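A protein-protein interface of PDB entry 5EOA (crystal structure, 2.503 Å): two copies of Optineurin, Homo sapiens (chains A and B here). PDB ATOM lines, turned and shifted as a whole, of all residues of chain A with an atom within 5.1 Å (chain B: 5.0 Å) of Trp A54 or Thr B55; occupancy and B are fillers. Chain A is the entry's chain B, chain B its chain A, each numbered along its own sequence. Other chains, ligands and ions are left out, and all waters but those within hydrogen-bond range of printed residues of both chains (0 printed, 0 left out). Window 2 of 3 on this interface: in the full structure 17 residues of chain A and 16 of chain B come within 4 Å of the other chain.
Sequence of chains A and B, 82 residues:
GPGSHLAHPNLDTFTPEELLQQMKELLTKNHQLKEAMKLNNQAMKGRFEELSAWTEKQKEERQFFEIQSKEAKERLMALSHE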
ATOM      1  N   GLU A  49      -8.826  -7.371  14.262  1.00  0.00           N
ATOM      2  CA  GLU A  49     -10.224  -7.108  14.535  1.00  0.00           C
ATOM      3  C   GLU A  49     -10.518  -7.108  16.043  1.00  0.00           C
ATOM      4  O   GLU A  49     -11.258  -6.247  16.527  1.00  0.00           O
ATOM      5  CB  GLU A  49     -11.099  -8.100  13.771  1.00  0.00           C
ATOM      6  CG  GLU A  49     -11.067  -7.852  12.264  1.00  0.00           C
ATOM      7  CD  GLU A  49     -11.605  -9.018  11.448  1.00  0.00           C
ATOM      8  OE1 GLU A  49     -11.809 -10.121  12.019  1.00  0.00           O
ATOM      9  OE2 GLU A  49     -11.820  -8.823  10.230  1.00  0.00           O
ATOM     10  N   GLU A  50      -9.916  -8.045  16.776  1.00  0.00           N
ATOM     11  CA  GLU A  50     -10.075  -8.100  18.228  1.00  0.00           C
ATOM     12  C   GLU A  50      -9.602  -6.820  18.927  1.00  0.00           C
ATOM     13  O   GLU A  50     -10.327  -6.249  19.740  1.00  0.00           O
ATOM     14  CB  GLU A  50      -9.369  -9.324  18.804  1.00  0.00           C
ATOM     15  CG  GLU A  50     -10.071 -10.634  18.476  1.00  0.00           C
ATOM     16  CD  GLU A  50      -9.241 -11.851  18.838  1.00  0.00           C
ATOM     17  OE1 GLU A  50      -8.122 -11.680  19.374  1.00  0.00           O
ATOM     18  OE2 GLU A  50      -9.706 -12.982  18.580  1.00  0.00           O
ATOM     19  N   LEU A  51      -8.395  -6.375  18.595  1.00  0.00           N
ATOM     20  CA  LEU A  51      -7.813  -5.164  19.157  1.00  0.00           C
ATOM     21  C   LEU A  51      -8.584  -3.915  18.745  1.00  0.00           C
ATOM     22  O   LEU A  51      -8.747  -2.966  19.529  1.00  0.00           O
ATOM     23  CB  LEU A  51      -6.386  -5.000  18.659  1.00  0.00           C
ATOM     24  CG  LEU A  51      -5.375  -5.994  19.178  1.00  0.00           C
ATOM     25  CD1 LEU A  51      -4.091  -5.782  18.411  1.00  0.00           C
ATOM     26  CD2 LEU A  51      -5.166  -5.779  20.664  1.00  0.00           C
ATOM     27  N   SER A  52      -9.029  -3.910  17.494  1.00  0.00           N
ATOM     28  CA  SER A  52      -9.832  -2.826  16.974  1.00  0.00           C
ATOM     29  C   SER A  52     -11.079  -2.647  17.863  1.00  0.00           C
ATOM     30  O   SER A  52     -11.300  -1.572  18.418  1.00  0.00           O
ATOM     31  CB  SER A  52     -10.206  -3.126  15.527  1.00  0.00           C
ATOM     32  OG  SER A  52     -10.950  -2.060  14.976  1.00  0.00           O
ATOM     33  N   ALA A  53     -11.852  -3.718  18.018  1.00  0.00           N
ATOM     34  CA  ALA A  53     -13.043  -3.726  18.850  1.00  0.00           C
ATOM     35  C   ALA A  53     -12.751  -3.285  20.286  1.00  0.00           C
ATOM     36  O   ALA A  53     -13.495  -2.500  20.879  1.00  0.00           O
ATOM     37  CB  ALA A  53     -13.660  -5.103  18.845  1.00  0.00           C
ATOM     38  N   TRP A  54     -11.651  -3.798  20.820  1.00  0.00           N
ATOM     39  CA  TRP A  54     -11.265  -3.623  22.211  1.00  0.00           C
ATOM     40  C   TRP A  54     -10.820  -2.191  22.515  1.00  0.00           C
ATOM     41  O   TRP A  54     -11.190  -1.614  23.538  1.00  0.00           O
ATOM     42  CB  TRP A  54     -10.157  -4.629  22.504  1.00  0.00           C
ATOM     43  CG  TRP A  54      -9.485  -4.544  23.825  1.00  0.00           C
ATOM     44  CD1 TRP A  54      -9.952  -5.008  25.023  1.00  0.00           C
ATOM     45  CD2 TRP A  54      -8.171  -4.037  24.077  1.00  0.00           C
ATOM     46  NE1 TRP A  54      -9.017  -4.788  26.010  1.00  0.00           N
ATOM     47  CE2 TRP A  54      -7.915  -4.195  25.451  1.00  0.00           C
ATOM     48  CE3 TRP A  54      -7.188  -3.455  23.272  1.00  0.00           C
ATOM     49  CZ2 TRP A  54      -6.716  -3.787  26.036  1.00  0.00           C
ATOM     50  CZ3 TRP A  54      -6.002  -3.056  23.852  1.00  0.00           C
ATOM     51  CH2 TRP A  54      -5.772  -3.226  25.219  1.00  0.00           C
ATOM     52  N   THR A  55     -10.020  -1.622  21.624  1.00  0.00           N
ATOM     53  CA  THR A  55      -9.618  -0.231  21.766  1.00  0.00           C
ATOM     54  C   THR A  55     -10.836   0.698  21.680  1.00  0.00           C
ATOM     55  O   THR A  55     -10.942   1.672  22.422  1.00  0.00           O
ATOM     56  CB  THR A  55      -8.593   0.139  20.687  1.00  0.00           C
ATOM     57  OG1 THR A  55      -9.143  -0.146  19.393  1.00  0.00           O
ATOM     58  CG2 THR A  55      -7.303  -0.669  20.882  1.00  0.00           C
ATOM     59  N   GLU A  56     -11.752   0.379  20.770  1.00  0.00           N
ATOM     60  CA  GLU A  56     -12.949   1.170  20.561  1.00  0.00           C
ATOM     61  C   GLU A  56     -13.783   1.154  21.844  1.00  0.00           C
ATOM     62  O   GLU A  56     -14.212   2.207  22.336  1.00  0.00           O
ATOM     63  CB  GLU A  56     -13.740   0.633  19.360  1.00  0.00           C
ATOM     64  CG  GLU A  56     -14.770   1.599  18.795  1.00  0.00           C
ATOM     65  CD  GLU A  56     -14.192   2.984  18.521  1.00  0.00           C
ATOM     66  OE1 GLU A  56     -13.045   3.074  18.022  1.00  0.00           O
ATOM     67  OE2 GLU A  56     -14.886   3.987  18.812  1.00  0.00           O
ATOM     68  N   LYS A  57     -13.967  -0.039  22.402  1.00  0.00           N
ATOM     69  CA  LYS A  57     -14.644  -0.172  23.674  1.00  0.00           C
ATOM     70  C   LYS A  57     -13.969   0.706  24.731  1.00  0.00           C
ATOM     71  O   LYS A  57     -14.659   1.467  25.405  1.00  0.00           O
ATOM     72  CB  LYS A  57     -14.720  -1.633  24.125  1.00  0.00           C
ATOM     73  CG  LYS A  57     -15.917  -1.919  25.033  1.00  0.00           C
ATOM     74  CD  LYS A  57     -15.940  -3.351  25.581  1.00  0.00           C
ATOM     75  CE  LYS A  57     -15.374  -3.439  26.996  1.00  0.00           C
ATOM     76  NZ  LYS A  57     -14.041  -2.765  27.133  1.00  0.00           N
ATOM     77  N   GLN A  58     -12.640   0.628  24.852  1.00  0.00           N
ATOM     78  CA  GLN A  58     -11.910   1.484  25.797  1.00  0.00           C
ATOM     79  C   GLN A  58     -12.224   2.973  25.601  1.00  0.00           C
ATOM     80  O   GLN A  58     -12.407   3.707  26.582  1.00  0.00           O
ATOM     81  CB  GLN A  58     -10.408   1.269  25.696  1.00  0.00           C
ATOM     82  CG  GLN A  58      -9.747   0.730  26.957  1.00  0.00           C
ATOM     83  CD  GLN A  58      -9.997  -0.738  27.153  1.00  0.00           C
ATOM     84  OE1 GLN A  58      -9.999  -1.503  26.194  1.00  0.00           O
ATOM     85  NE2 GLN A  58     -10.224  -1.144  28.396  1.00  0.00           N
ATOM     86  N   LEU B  51       0.325  -0.780  22.928  1.00  0.00           N
ATOM     87  CA  LEU B  51      -1.073  -1.049  23.249  1.00  0.00           C
ATOM     88  C   LEU B  51      -1.281  -1.322  24.739  1.00  0.00           C
ATOM     89  O   LEU B  51      -2.263  -0.865  25.332  1.00  0.00           O
ATOM     90  CB  LEU B  51      -1.631  -2.188  22.402  1.00  0.00           C
ATOM     91  CG  LEU B  51      -1.839  -1.797  20.944  1.00  0.00           C
ATOM     92  CD1 LEU B  51      -1.972  -3.037  20.081  1.00  0.00           C
ATOM     93  CD2 LEU B  51      -3.074  -0.929  20.801  1.00  0.00           C
ATOM     94  N   SER B  52      -0.353  -2.052  25.344  1.00  0.00           N
ATOM     95  CA  SER B  52      -0.399  -2.290  26.780  1.00  0.00           C
ATOM     96  C   SER B  52      -0.366  -0.961  27.511  1.00  0.00           C
ATOM     97  O   SER B  52      -1.188  -0.707  28.389  1.00  0.00           O
ATOM     98  CB  SER B  52       0.782  -3.143  27.226  1.00  0.00           C
ATOM     99  OG  SER B  52       0.682  -4.439  26.689  1.00  0.00           O
ATOM    100  N   ALA B  53       0.578  -0.112  27.133  1.00  0.00           N
ATOM    101  CA  ALA B  53       0.748   1.159  27.795  1.00  0.00           C
ATOM    102  C   ALA B  53      -0.542   1.984  27.651  1.00  0.00           C
ATOM    103  O   ALA B  53      -1.070   2.515  28.631  1.00  0.00           O
ATOM    104  CB  ALA B  53       1.931   1.895  27.212  1.00  0.00           C
ATOM    105  N   TRP B  54      -1.051   2.040  26.423  1.00  0.00           N
ATOM    106  CA  TRP B  54      -2.210   2.834  26.071  1.00  0.00           C
ATOM    107  C   TRP B  54      -3.446   2.498  26.887  1.00  0.00           C
ATOM    108  O   TRP B  54      -4.155   3.402  27.353  1.00  0.00           O
ATOM    109  CB  TRP B  54      -2.528   2.632  24.595  1.00  0.00           C
ATOM    110  CG  TRP B  54      -3.726   3.408  24.117  1.00  0.00           C
ATOM    111  CD1 TRP B  54      -3.744   4.701  23.680  1.00  0.00           C
ATOM    112  CD2 TRP B  54      -5.072   2.931  24.010  1.00  0.00           C
ATOM    113  NE1 TRP B  54      -5.013   5.057  23.300  1.00  0.00           N
ATOM    114  CE2 TRP B  54      -5.850   3.992  23.495  1.00  0.00           C
ATOM    115  CE3 TRP B  54      -5.696   1.714  24.295  1.00  0.00           C
ATOM    116  CZ2 TRP B  54      -7.220   3.873  23.264  1.00  0.00           C
ATOM    117  CZ3 TRP B  54      -7.059   1.592  24.059  1.00  0.00           C
ATOM    118  CH2 TRP B  54      -7.805   2.666  23.548  1.00  0.00           C
ATOM    119  N   THR B  55      -3.718   1.201  27.024  1.00  0.00           N
ATOM    120  CA  THR B  55      -4.936   0.760  27.673  1.00  0.00           C
ATOM    121  C   THR B  55      -4.858   1.056  29.164  1.00  0.00           C
ATOM    122  O   THR B  55      -5.842   1.486  29.774  1.00  0.00           O
ATOM    123  CB  THR B  55      -5.229  -0.711  27.386  1.00  0.00           C
ATOM    124  OG1 THR B  55      -6.469  -1.082  27.992  1.00  0.00           O
ATOM    125  CG2 THR B  55      -4.143  -1.598  27.928  1.00  0.00           C
ATOM    126  N   GLU B  56      -3.671   0.858  29.727  1.00  0.00           N
ATOM    127  CA  GLU B  56      -3.393   1.224  31.099  1.00  0.00           C
ATOM    128  C   GLU B  56      -3.665   2.705  31.306  1.00  0.00           C
ATOM    129  O   GLU B  56      -4.225   3.112  32.324  1.00  0.00           O
ATOM    130  CB  GLU B  56      -1.935   0.935  31.419  1.00  0.00           C
ATOM    131  CG  GLU B  56      -1.736   0.298  32.764  1.00  0.00           C
ATOM    132  CD  GLU B  56      -2.483  -1.015  32.883  1.00  0.00           C
ATOM    133  OE1 GLU B  56      -3.216  -1.195  33.880  1.00  0.00           O
ATOM    134  OE2 GLU B  56      -2.338  -1.863  31.974  1.00  0.00           O
ATOM    135  N   LYS B  57      -3.260   3.513  30.338  1.00  0.00           N
ATOM    136  CA  LYS B  57      -3.498   4.940  30.412  1.00  0.00           C
ATOM    137  C   LYS B  57      -4.994   5.239  30.331  1.00  0.00           C
ATOM    138  O   LYS B  57      -5.495   6.085  31.074  1.00  0.00           O
ATOM    139  CB  LYS B  57      -2.730   5.663  29.310  1.00  0.00           C
ATOM    140  CG  LYS B  57      -3.008   7.147  29.206  1.00  0.00           C
ATOM    141  CD  LYS B  57      -2.613   7.645  27.823  1.00  0.00           C
ATOM    142  CE  LYS B  57      -3.104   9.052  27.556  1.00  0.00           C
ATOM    143  NZ  LYS B  57      -2.442  10.027  28.441  1.00  0.00           N
ATOM    144  N   GLN B  58      -5.713   4.540  29.452  1.00  0.00           N
ATOM    145  CA  GLN B  58      -7.147   4.764  29.329  1.00  0.00           C
ATOM    146  C   GLN B  58      -7.834   4.406  30.636  1.00  0.00           C
ATOM    147  O   GLN B  58      -8.646   5.186  31.138  1.00  0.00           O
ATOM    148  CB  GLN B  58      -7.764   3.954  28.191  1.00  0.00           C
ATOM    149  CG  GLN B  58      -7.239   4.280  26.809  1.00  0.00           C
ATOM    150  CD  GLN B  58      -7.349   5.737  26.462  1.00  0.00           C
ATOM    151  OE1 GLN B  58      -8.445   6.253  26.262  1.00  0.00           O
ATOM    152  NE2 GLN B  58      -6.210   6.415  26.387  1.00  0.00           N
ATOM    153  N   LYS B  59      -7.505   3.232  31.181  1.00  0.00           N
ATOM    154  CA  LYS B  59      -8.091   2.786  32.439  1.00  0.00           C
ATOM    155  C   LYS B  59      -7.914   3.814  33.534  1.00  0.00           C
ATOM    156  O   LYS B  59      -8.863   4.126  34.248  1.00  0.00           O
ATOM    157  CB  LYS B  59      -7.515   1.450  32.897  1.00  0.00           C
ATOM    158  CG  LYS B  59      -8.152   0.255  32.207  1.00  0.00           C
ATOM    159  CD  LYS B  59      -7.756  -1.053  32.888  1.00  0.00           C
ATOM    160  CE  LYS B  59      -8.640  -2.209  32.431  1.00  0.00           C
ATOM    161  NZ  LYS B  59      -8.617  -3.335  33.418  1.00  0.00           N
ATOM    162  N   GLU B  60      -6.700   4.341  33.650  1.00  0.00           N
ATOM    163  CA  GLU B  60      -6.404   5.331  34.669  1.00  0.00           C
ATOM    164  C   GLU B  60      -7.260   6.576  34.480  1.00  0.00           C
ATOM    165  O   GLU B  60      -7.912   7.039  35.416  1.00  0.00           O
ATOM    166  CB  GLU B  60      -4.922   5.678  34.662  1.00  0.00           C
ATOM    167  CG  GLU B  60      -4.073   4.532  35.163  1.00  0.00           C
ATOM    168  CD  GLU B  60      -2.590   4.833  35.138  1.00  0.00           C
ATOM    169  OE1 GLU B  60      -2.228   6.007  34.889  1.00  0.00           O
ATOM    170  OE2 GLU B  60      -1.791   3.891  35.371  1.00  0.00           O
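The side-chain hydroxyl (OG1) of Thr A55 sits at hydrogen-bond distance from the backbone carbonyl oxygen (O) of Ser A52 (2.8 Å).
O of Trp A54 lies close to OE1 of Gln A58 (2.9 Å).
The backbone carbonyl oxygen (O) of Leu A51 lies within hydrogen-bond range of the side-chain hydroxyl (OG1) of Thr A55 (2.9 Å).
Among the printed residues, merely in contact across the chains: Leu A51 with Leu B51, Trp A54 with Thr B55, Thr A55 with Trp B54, Gln A58 with Trp B54, Gln A58 with Thr B55 and Gln A58 with Gln B58.
Leu B51 touches its own counterpart, Leu A51.
Trp A54 touches Thr B55, and with the chains exchanged Thr A55 touches Trp B54.
Gln A58 touches Trp B54, but with the chains exchanged Trp A54 does not touch Gln B58 (7.8 Å).
Gln B58 touches its own counterpart, Gln A58.
Positions printed for both chains: 51, 52, 53, 54, 55, 56, 57 and 58.
Along chain A the printed residues that touch a printed residue of chain B span positions 51 to 58.
Printed residues of chain B that touch a printed residue of chain A: Leu B51, Trp B54, Thr B55 and Gln B58.
Hydrophobic or aromatic side chains of chain B that line the printed part of chain A: Leu B51 and Trp B54.
Among the printed residues, 6 pairs touch across the chains.
Among the printed residues, no Asp or Glu carboxylate lies within 4 Å of a Lys or Arg side-chain nitrogen of the other chain.
Printed residues of chain B within 4 Å of Leu A51: Leu B51.
Trp A54 touches just one residue of chain B: Thr B55.
Of the printed residues of chain B, Thr A55 touches Trp B54.
Lys A57 touches none of the printed residues of chain B.
Of the printed residues of chain B, Gln A58 touches Trp B54 (3.7 Å), Thr B55 (3.6 Å) and Gln B58 (3.98 Å).
Of the printed residues of chain A, Leu B51 touches Leu A51 (3.8 Å).
Ser B52 touches none of the printed residues of chain A.
Of the printed residues of chain A, Trp B54 touches Thr A55 (3.5 Å) and Gln A58 (3.7 Å).
The nearest residue of chain B that does not touch Trp A54 is Leu B51 (4.2 Å).
The nearest printed residue of chain A that does not touch Gln B58 is Thr A55 (6.3 Å).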
